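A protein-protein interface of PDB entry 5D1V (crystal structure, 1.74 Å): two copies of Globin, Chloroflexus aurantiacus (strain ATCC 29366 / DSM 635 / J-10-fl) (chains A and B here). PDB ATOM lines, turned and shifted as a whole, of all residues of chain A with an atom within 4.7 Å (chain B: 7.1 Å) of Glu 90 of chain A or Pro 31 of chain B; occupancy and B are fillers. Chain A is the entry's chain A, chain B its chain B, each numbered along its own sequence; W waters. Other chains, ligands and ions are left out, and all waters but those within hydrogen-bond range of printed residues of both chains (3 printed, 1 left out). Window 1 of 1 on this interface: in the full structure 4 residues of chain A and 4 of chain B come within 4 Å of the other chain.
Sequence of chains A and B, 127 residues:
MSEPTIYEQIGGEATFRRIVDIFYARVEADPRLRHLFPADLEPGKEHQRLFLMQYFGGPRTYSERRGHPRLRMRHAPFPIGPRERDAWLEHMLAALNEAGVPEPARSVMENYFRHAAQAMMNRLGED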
ATOM      1  N   ARG A  26     -17.229  28.018  -3.095  1.00  0.00           N
ATOM      2  CA  ARG A  26     -17.542  27.187  -1.948  1.00  0.00           C
ATOM      3  C   ARG A  26     -18.464  27.910  -0.979  1.00  0.00           C
ATOM      4  O   ARG A  26     -19.413  27.330  -0.486  1.00  0.00           O
ATOM      5  CB  ARG A  26     -16.236  26.750  -1.260  1.00  0.00           C
ATOM      6  CG  ARG A  26     -15.451  25.844  -2.165  1.00  0.00           C
ATOM      7  CD  ARG A  26     -14.097  25.494  -1.645  1.00  0.00           C
ATOM      8  NE  ARG A  26     -14.291  24.669  -0.474  1.00  0.00           N
ATOM      9  CZ  ARG A  26     -14.015  23.377  -0.381  1.00  0.00           C
ATOM     10  NH1 ARG A  26     -13.469  22.705  -1.382  1.00  0.00           N
ATOM     11  NH2 ARG A  26     -14.281  22.766   0.756  1.00  0.00           N
ATOM     12  N   ARG A  32     -24.158  27.107   5.492  1.00  0.00           N
ATOM     13  CA  ARG A  32     -23.673  27.582   6.792  1.00  0.00           C
ATOM     14  C   ARG A  32     -23.248  29.032   6.726  1.00  0.00           C
ATOM     15  O   ARG A  32     -23.259  29.723   7.742  1.00  0.00           O
ATOM     16  CB  ARG A  32     -22.499  26.733   7.271  1.00  0.00           C
ATOM     17  CG  ARG A  32     -22.831  25.276   7.464  1.00  0.00           C
ATOM     18  CD  ARG A  32     -21.605  24.531   7.907  1.00  0.00           C
ATOM     19  NE  ARG A  32     -20.652  24.352   6.817  1.00  0.00           N
ATOM     20  CZ  ARG A  32     -19.446  23.824   6.960  1.00  0.00           C
ATOM     21  NH1 ARG A  32     -19.019  23.444   8.153  1.00  0.00           N
ATOM     22  NH2 ARG A  32     -18.654  23.691   5.908  1.00  0.00           N
ATOM     23  N   ASP A  86     -15.323  27.505  11.555  1.00  0.00           N
ATOM     24  CA  ASP A  86     -14.954  26.217  10.989  1.00  0.00           C
ATOM     25  C   ASP A  86     -15.296  26.155   9.499  1.00  0.00           C
ATOM     26  O   ASP A  86     -14.501  25.676   8.689  1.00  0.00           O
ATOM     27  CB  ASP A  86     -15.650  25.060  11.719  1.00  0.00           C
ATOM     28  CG  ASP A  86     -15.098  24.795  13.095  1.00  0.00           C
ATOM     29  OD1 ASP A  86     -14.104  25.427  13.477  1.00  0.00           O
ATOM     30  OD2 ASP A  86     -15.675  23.920  13.785  1.00  0.00           O
ATOM     31  N   ALA A  87     -16.467  26.655   9.127  1.00  0.00           N
ATOM     32  CA  ALA A  87     -16.869  26.644   7.726  1.00  0.00           C
ATOM     33  C   ALA A  87     -15.965  27.548   6.876  1.00  0.00           C
ATOM     34  O   ALA A  87     -15.486  27.137   5.831  1.00  0.00           O
ATOM     35  CB  ALA A  87     -18.344  27.047   7.583  1.00  0.00           C
ATOM     36  N   TRP A  88     -15.696  28.768   7.339  1.00  0.00           N
ATOM     37  CA  TRP A  88     -14.817  29.663   6.626  1.00  0.00           C
ATOM     38  C   TRP A  88     -13.422  29.042   6.401  1.00  0.00           C
ATOM     39  O   TRP A  88     -12.880  29.022   5.282  1.00  0.00           O
ATOM     40  CB  TRP A  88     -14.711  30.962   7.414  1.00  0.00           C
ATOM     41  CG  TRP A  88     -14.123  32.071   6.636  1.00  0.00           C
ATOM     42  CD1 TRP A  88     -14.796  33.068   5.996  1.00  0.00           C
ATOM     43  CD2 TRP A  88     -12.731  32.316   6.402  1.00  0.00           C
ATOM     44  NE1 TRP A  88     -13.919  33.919   5.400  1.00  0.00           N
ATOM     45  CE2 TRP A  88     -12.649  33.485   5.618  1.00  0.00           C
ATOM     46  CE3 TRP A  88     -11.544  31.683   6.802  1.00  0.00           C
ATOM     47  CZ2 TRP A  88     -11.428  34.028   5.204  1.00  0.00           C
ATOM     48  CZ3 TRP A  88     -10.335  32.220   6.380  1.00  0.00           C
ATOM     49  CH2 TRP A  88     -10.295  33.376   5.580  1.00  0.00           C
ATOM     50  N   LEU A  89     -12.860  28.502   7.468  1.00  0.00           N
ATOM     51  CA  LEU A  89     -11.498  27.958   7.429  1.00  0.00           C
ATOM     52  C   LEU A  89     -11.441  26.738   6.516  1.00  0.00           C
ATOM     53  O   LEU A  89     -10.489  26.582   5.751  1.00  0.00           O
ATOM     54  CB  LEU A  89     -11.037  27.609   8.834  1.00  0.00           C
ATOM     55  CG  LEU A  89      -9.553  27.497   9.076  1.00  0.00           C
ATOM     56  CD1 LEU A  89      -8.843  28.802   8.720  1.00  0.00           C
ATOM     57  CD2 LEU A  89      -9.374  27.170  10.537  1.00  0.00           C
ATOM     58  N   GLU A  90     -12.465  25.886   6.568  1.00  0.00           N
ATOM     59  CA  GLU A  90     -12.533  24.738   5.657  1.00  0.00           C
ATOM     60  C   GLU A  90     -12.350  25.193   4.207  1.00  0.00           C
ATOM     61  O   GLU A  90     -11.543  24.631   3.440  1.00  0.00           O
ATOM     62  CB  GLU A  90     -13.868  23.997   5.805  1.00  0.00           C
ATOM     63  CG  GLU A  90     -14.044  22.867   4.802  1.00  0.00           C
ATOM     64  CD  GLU A  90     -15.388  22.171   4.875  1.00  0.00           C
ATOM     65  OE1 GLU A  90     -16.072  22.270   5.920  1.00  0.00           O
ATOM     66  OE2 GLU A  90     -15.735  21.466   3.900  1.00  0.00           O
ATOM     67  N   HIS A  91     -13.114  26.208   3.824  1.00  0.00           N
ATOM     68  CA  HIS A  91     -13.127  26.602   2.432  1.00  0.00           C
ATOM     69  C   HIS A  91     -11.879  27.368   2.050  1.00  0.00           C
ATOM     70  O   HIS A  91     -11.393  27.214   0.935  1.00  0.00           O
ATOM     71  CB  HIS A  91     -14.384  27.404   2.133  1.00  0.00           C
ATOM     72  CG  HIS A  91     -15.633  26.616   2.351  1.00  0.00           C
ATOM     73  ND1 HIS A  91     -15.766  25.311   1.927  1.00  0.00           N
ATOM     74  CD2 HIS A  91     -16.802  26.938   2.949  1.00  0.00           C
ATOM     75  CE1 HIS A  91     -16.959  24.862   2.265  1.00  0.00           C
ATOM     76  NE2 HIS A  91     -17.605  25.829   2.888  1.00  0.00           N
ATOM     77  N   MET A  92     -11.326  28.164   2.965  1.00  0.00           N
ATOM     78  CA  MET A  92     -10.125  28.908   2.600  1.00  0.00           C
ATOM     79  C   MET A  92      -8.943  27.969   2.551  1.00  0.00           C
ATOM     80  O   MET A  92      -8.066  28.084   1.685  1.00  0.00           O
ATOM     81  CB  MET A  92      -9.814  30.061   3.561  1.00  0.00           C
ATOM     82  CG  MET A  92      -8.595  30.910   3.076  1.00  0.00           C
ATOM     83  SD  MET A  92      -8.867  31.717   1.463  1.00  0.00           S
ATOM     84  CE  MET A  92      -9.991  33.021   1.906  1.00  0.00           C
ATOM     85  N   LEU A  93      -8.868  27.029   3.477  1.00  0.00           N
ATOM     86  CA  LEU A  93      -7.766  26.087   3.370  1.00  0.00           C
ATOM     87  C   LEU A  93      -7.861  25.261   2.084  1.00  0.00           C
ATOM     88  O   LEU A  93      -6.845  24.994   1.436  1.00  0.00           O
ATOM     89  CB  LEU A  93      -7.725  25.190   4.604  1.00  0.00           C
ATOM     90  CG  LEU A  93      -7.447  26.003   5.865  1.00  0.00           C
ATOM     91  CD1 LEU A  93      -7.291  25.059   7.060  1.00  0.00           C
ATOM     92  CD2 LEU A  93      -6.246  26.915   5.748  1.00  0.00           C
ATOM     93  N   ALA A  94      -9.065  24.847   1.707  1.00  0.00           N
ATOM     94  CA  ALA A  94      -9.231  24.107   0.460  1.00  0.00           C
ATOM     95  C   ALA A  94      -8.813  24.965  -0.723  1.00  0.00           C
ATOM     96  O   ALA A  94      -8.177  24.477  -1.663  1.00  0.00           O
ATOM     97  CB  ALA A  94     -10.672  23.636   0.302  1.00  0.00           C
ATOM     98  N   ARG B  26      -3.578  15.474  11.853  1.00  0.00           N
ATOM     99  CA  ARG B  26      -4.382  15.839  10.678  1.00  0.00           C
ATOM    100  C   ARG B  26      -5.851  16.097  11.050  1.00  0.00           C
ATOM    101  O   ARG B  26      -6.466  17.060  10.566  1.00  0.00           O
ATOM    102  CB  ARG B  26      -4.244  14.742   9.630  1.00  0.00           C
ATOM    103  CG  ARG B  26      -2.872  14.762   8.967  1.00  0.00           C
ATOM    104  CD  ARG B  26      -2.737  13.604   8.022  1.00  0.00           C
ATOM    105  NE  ARG B  26      -3.592  13.856   6.873  1.00  0.00           N
ATOM    106  CZ  ARG B  26      -3.176  14.329   5.706  1.00  0.00           C
ATOM    107  NH1 ARG B  26      -1.879  14.576   5.485  1.00  0.00           N
ATOM    108  NH2 ARG B  26      -4.069  14.536   4.754  1.00  0.00           N
ATOM    109  N   VAL B  27      -6.398  15.266  11.934  1.00  0.00           N
ATOM    110  CA  VAL B  27      -7.765  15.403  12.425  1.00  0.00           C
ATOM    111  C   VAL B  27      -7.901  16.726  13.167  1.00  0.00           C
ATOM    112  O   VAL B  27      -8.845  17.497  12.939  1.00  0.00           O
ATOM    113  CB  VAL B  27      -8.142  14.222  13.334  1.00  0.00           C
ATOM    114  CG1 VAL B  27      -9.426  14.513  14.076  1.00  0.00           C
ATOM    115  CG2 VAL B  27      -8.289  12.924  12.525  1.00  0.00           C
ATOM    116  N   GLU B  28      -6.932  17.002  14.037  1.00  0.00           N
ATOM    117  CA  GLU B  28      -7.004  18.193  14.864  1.00  0.00           C
ATOM    118  C   GLU B  28      -7.012  19.445  13.997  1.00  0.00           C
ATOM    119  O   GLU B  28      -7.669  20.452  14.336  1.00  0.00           O
ATOM    120  CB  GLU B  28      -5.832  18.191  15.851  1.00  0.00           C
ATOM    121  CG  GLU B  28      -5.811  19.347  16.797  1.00  0.00           C
ATOM    122  CD  GLU B  28      -4.737  19.179  17.862  1.00  0.00           C
ATOM    123  OE1 GLU B  28      -3.712  18.502  17.596  1.00  0.00           O
ATOM    124  OE2 GLU B  28      -4.931  19.700  18.968  1.00  0.00           O
ATOM    125  N   ALA B  29      -6.285  19.385  12.881  1.00  0.00           N
ATOM    126  CA  ALA B  29      -6.143  20.521  11.962  1.00  0.00           C
ATOM    127  C   ALA B  29      -7.275  20.625  10.928  1.00  0.00           C
ATOM    128  O   ALA B  29      -7.287  21.565  10.134  1.00  0.00           O
ATOM    129  CB  ALA B  29      -4.843  20.445  11.241  1.00  0.00           C
ATOM    130  N   ASP B  30      -8.212  19.677  10.936  1.00  0.00           N
ATOM    131  CA  ASP B  30      -9.243  19.596   9.899  1.00  0.00           C
ATOM    132  C   ASP B  30     -10.609  20.080  10.397  1.00  0.00           C
ATOM    133  O   ASP B  30     -11.289  19.363  11.132  1.00  0.00           O
ATOM    134  CB  ASP B  30      -9.359  18.151   9.415  1.00  0.00           C
ATOM    135  CG  ASP B  30     -10.328  18.003   8.272  1.00  0.00           C
ATOM    136  OD1 ASP B  30     -10.949  19.008   7.847  1.00  0.00           O
ATOM    137  OD2 ASP B  30     -10.477  16.869   7.797  1.00  0.00           O
ATOM    138  N   PRO B  31     -11.028  21.295   9.993  1.00  0.00           N
ATOM    139  CA  PRO B  31     -12.327  21.747  10.504  1.00  0.00           C
ATOM    140  C   PRO B  31     -13.516  20.897  10.044  1.00  0.00           C
ATOM    141  O   PRO B  31     -14.610  21.098  10.575  1.00  0.00           O
ATOM    142  CB  PRO B  31     -12.434  23.199   9.980  1.00  0.00           C
ATOM    143  CG  PRO B  31     -11.352  23.356   8.980  1.00  0.00           C
ATOM    144  CD  PRO B  31     -10.302  22.345   9.258  1.00  0.00           C
ATOM    145  N   ARG B  32     -13.329  19.962   9.115  1.00  0.00           N
ATOM    146  CA  ARG B  32     -14.389  19.018   8.765  1.00  0.00           C
ATOM    147  C   ARG B  32     -14.664  18.045   9.910  1.00  0.00           C
ATOM    148  O   ARG B  32     -15.768  17.492  10.020  1.00  0.00           O
ATOM    149  CB  ARG B  32     -14.031  18.225   7.508  1.00  0.00           C
ATOM    150  CG  ARG B  32     -13.834  19.087   6.269  1.00  0.00           C
ATOM    151  CD  ARG B  32     -13.435  18.232   5.062  1.00  0.00           C
ATOM    152  NE  ARG B  32     -12.096  17.702   5.227  1.00  0.00           N
ATOM    153  CZ  ARG B  32     -11.500  16.859   4.398  1.00  0.00           C
ATOM    154  NH1 ARG B  32     -12.140  16.408   3.331  1.00  0.00           N
ATOM    155  NH2 ARG B  32     -10.261  16.452   4.648  1.00  0.00           N
ATOM    156  N   LEU B  33     -13.679  17.866  10.782  1.00  0.00           N
ATOM    157  CA  LEU B  33     -13.743  16.798  11.782  1.00  0.00           C
ATOM    158  C   LEU B  33     -13.562  17.221  13.220  1.00  0.00           C
ATOM    159  O   LEU B  33     -14.084  16.559  14.104  1.00  0.00           O
ATOM    160  CB  LEU B  33     -12.683  15.737  11.479  1.00  0.00           C
ATOM    161  CG  LEU B  33     -12.855  14.876  10.249  1.00  0.00           C
ATOM    162  CD1 LEU B  33     -11.653  13.939  10.136  1.00  0.00           C
ATOM    163  CD2 LEU B  33     -14.118  14.094  10.356  1.00  0.00           C
ATOM    164  N   ARG B  34     -12.810  18.302  13.467  1.00  0.00           N
ATOM    165  CA  ARG B  34     -12.384  18.632  14.827  1.00  0.00           C
ATOM    166  C   ARG B  34     -13.565  18.734  15.770  1.00  0.00           C
ATOM    167  O   ARG B  34     -13.487  18.335  16.937  1.00  0.00           O
ATOM    168  CB  ARG B  34     -11.598  19.958  14.863  1.00  0.00           C
ATOM    169  CG  ARG B  34     -11.226  20.452  16.297  1.00  0.00           C
ATOM    170  CD  ARG B  34     -10.217  19.518  16.849  1.00  0.00           C
ATOM    171  NE  ARG B  34      -9.793  19.744  18.245  1.00  0.00           N
ATOM    172  CZ  ARG B  34     -10.390  19.236  19.324  1.00  0.00           C
ATOM    173  NH1 ARG B  34     -11.513  18.547  19.225  1.00  0.00           N
ATOM    174  NH2 ARG B  34      -9.862  19.439  20.518  1.00  0.00           N
ATOM    175  N   HIS B  35     -14.673  19.256  15.257  1.00  0.00           N
ATOM    176  CA  HIS B  35     -15.823  19.543  16.095  1.00  0.00           C
ATOM    177  C   HIS B  35     -16.434  18.282  16.716  1.00  0.00           C
ATOM    178  O   HIS B  35     -17.116  18.360  17.734  1.00  0.00           O
ATOM    179  CB  HIS B  35     -16.889  20.285  15.293  1.00  0.00           C
ATOM    180  CG  HIS B  35     -17.480  19.486  14.175  1.00  0.00           C
ATOM    181  ND1 HIS B  35     -18.702  18.857  14.271  1.00  0.00           N
ATOM    182  CD2 HIS B  35     -17.030  19.239  12.922  1.00  0.00           C
ATOM    183  CE1 HIS B  35     -18.972  18.247  13.132  1.00  0.00           C
ATOM    184  NE2 HIS B  35     -17.971  18.453  12.299  1.00  0.00           N
ATOM    185  N   LEU B  36     -16.177  17.131  16.108  1.00  0.00           N
ATOM    186  CA  LEU B  36     -16.743  15.876  16.600  1.00  0.00           C
ATOM    187  C   LEU B  36     -15.998  15.346  17.790  1.00  0.00           C
ATOM    188  O   LEU B  36     -16.542  14.549  18.534  1.00  0.00           O
ATOM    189  CB  LEU B  36     -16.738  14.811  15.508  1.00  0.00           C
ATOM    190  CG  LEU B  36     -17.582  15.111  14.284  1.00  0.00           C
ATOM    191  CD1 LEU B  36     -17.278  14.092  13.207  1.00  0.00           C
ATOM    192  CD2 LEU B  36     -19.069  15.091  14.664  1.00  0.00           C
ATOM    193  N   ARG B  83     -18.988  12.765   3.800  1.00  0.00           N
ATOM    194  CA  ARG B  83     -18.061  13.869   4.114  1.00  0.00           C
ATOM    195  C   ARG B  83     -17.043  13.501   5.191  1.00  0.00           C
ATOM    196  O   ARG B  83     -15.813  13.611   5.000  1.00  0.00           O
ATOM    197  CB  ARG B  83     -18.879  15.059   4.562  1.00  0.00           C
ATOM    198  CG  ARG B  83     -18.095  16.235   5.087  1.00  0.00           C
ATOM    199  CD  ARG B  83     -19.068  17.354   5.388  1.00  0.00           C
ATOM    200  NE  ARG B  83     -18.569  18.288   6.385  1.00  0.00           N
ATOM    201  CZ  ARG B  83     -17.815  19.343   6.102  1.00  0.00           C
ATOM    202  NH1 ARG B  83     -17.454  19.584   4.852  1.00  0.00           N
ATOM    203  NH2 ARG B  83     -17.428  20.158   7.077  1.00  0.00           N
HETATM  204  O   HOH W   1     -14.513  21.403  13.224  1.00  0.00           O
HETATM  205  O   HOH W   2     -17.345  21.518  10.356  1.00  0.00           O
HETATM  206  O   HOH W   3     -18.643  21.874   3.134  1.00  0.00           O
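Water W1 lies within hydrogen-bond range of O of Pro 31 of chain B (2.7 Å), OD2 of Asp 86 of chain A (2.8 Å) and N of His 35 of chain B (3.0 Å).
Water W2 bridges the backbone carbonyl oxygen of Pro 31 of chain B and the guanidinium group of Arg 32 of chain A.
Water W3 lies within hydrogen-bond range of OE2 of Glu 90 of chain A (3.0 Å), NH1 of Arg 83 of chain B (3.1 Å) and NH2 of Arg 32 of chain A (3.3 Å).
Of the 12 printed residues of chain B, 3 touch a printed residue of chain A.
Among the printed residues, 5 pairs touch across the chains.
Among the printed residues, Asp or Glu carboxylates within 4 Å of a Lys or Arg side-chain nitrogen of the other chain: Glu 90 of chain A with Arg 83 of chain B.
The guanidinium group (NH1) of Arg 83 of chain B lies within salt-bridge range of the side-chain carboxylate (OE2) of Glu 90 of chain A (2.7 Å).
Of the printed residues of chain B, Arg 32 of chain A touches Arg 83.
Printed residues of chain B within 4 Å of Asp 86 of chain A: Pro 31.
Of chain B, only Pro 31, Arg 32 and Arg 83 come within 4 Å of Glu 90 of chain A.
Of chain A, only Asp 86 and Glu 90 come within 4 Å of Pro 31 of chain B.
Printed residues of chain A within 4 Å of Arg 32 of chain B: Glu 90.
Of the printed residues of chain A, Arg 83 of chain B touches Arg 32 and Glu 90.
The nearest residue of chain B that does not touch Glu 90 of chain A is Asp 30 of chain B (5.8 Å).
Among the printed residues, pairs that only touch across the chains: Asp 86 of chain A with Pro 31 of chain B (3.5 Å), Glu 90 of chain A with Pro 31 of chain B (3.7 Å), Glu 90 of chain A with Arg 32 of chain B (3.7 Å) and Arg 32 of chain A with Arg 83 of chain B (3.8 Å).
2 positions are printed for both chains.
Of the 5 pairs that touch across the chains among the printed residues, none has its exchanged pair printed and touching as well.
The guanidinium group of Arg 26 of chain A lies within salt-bridge range of the side-chain carboxylate of Glu 90 of chain A (3.7 Å).
O of Arg 32 of chain B sits at hydrogen-bond distance from NE2 of His 35 of chain B.
The side-chain carboxylate (OD1) of Asp 30 of chain B lies within salt-bridge range of the guanidinium group (NE) of Arg 32 of chain B, at 3.1 Å.
The guanidinium group (NH2) of Arg 32 of chain A is in salt-bridge range of the side-chain carboxylate (OE1) of Glu 90 of chain A, at 2.9 Å.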
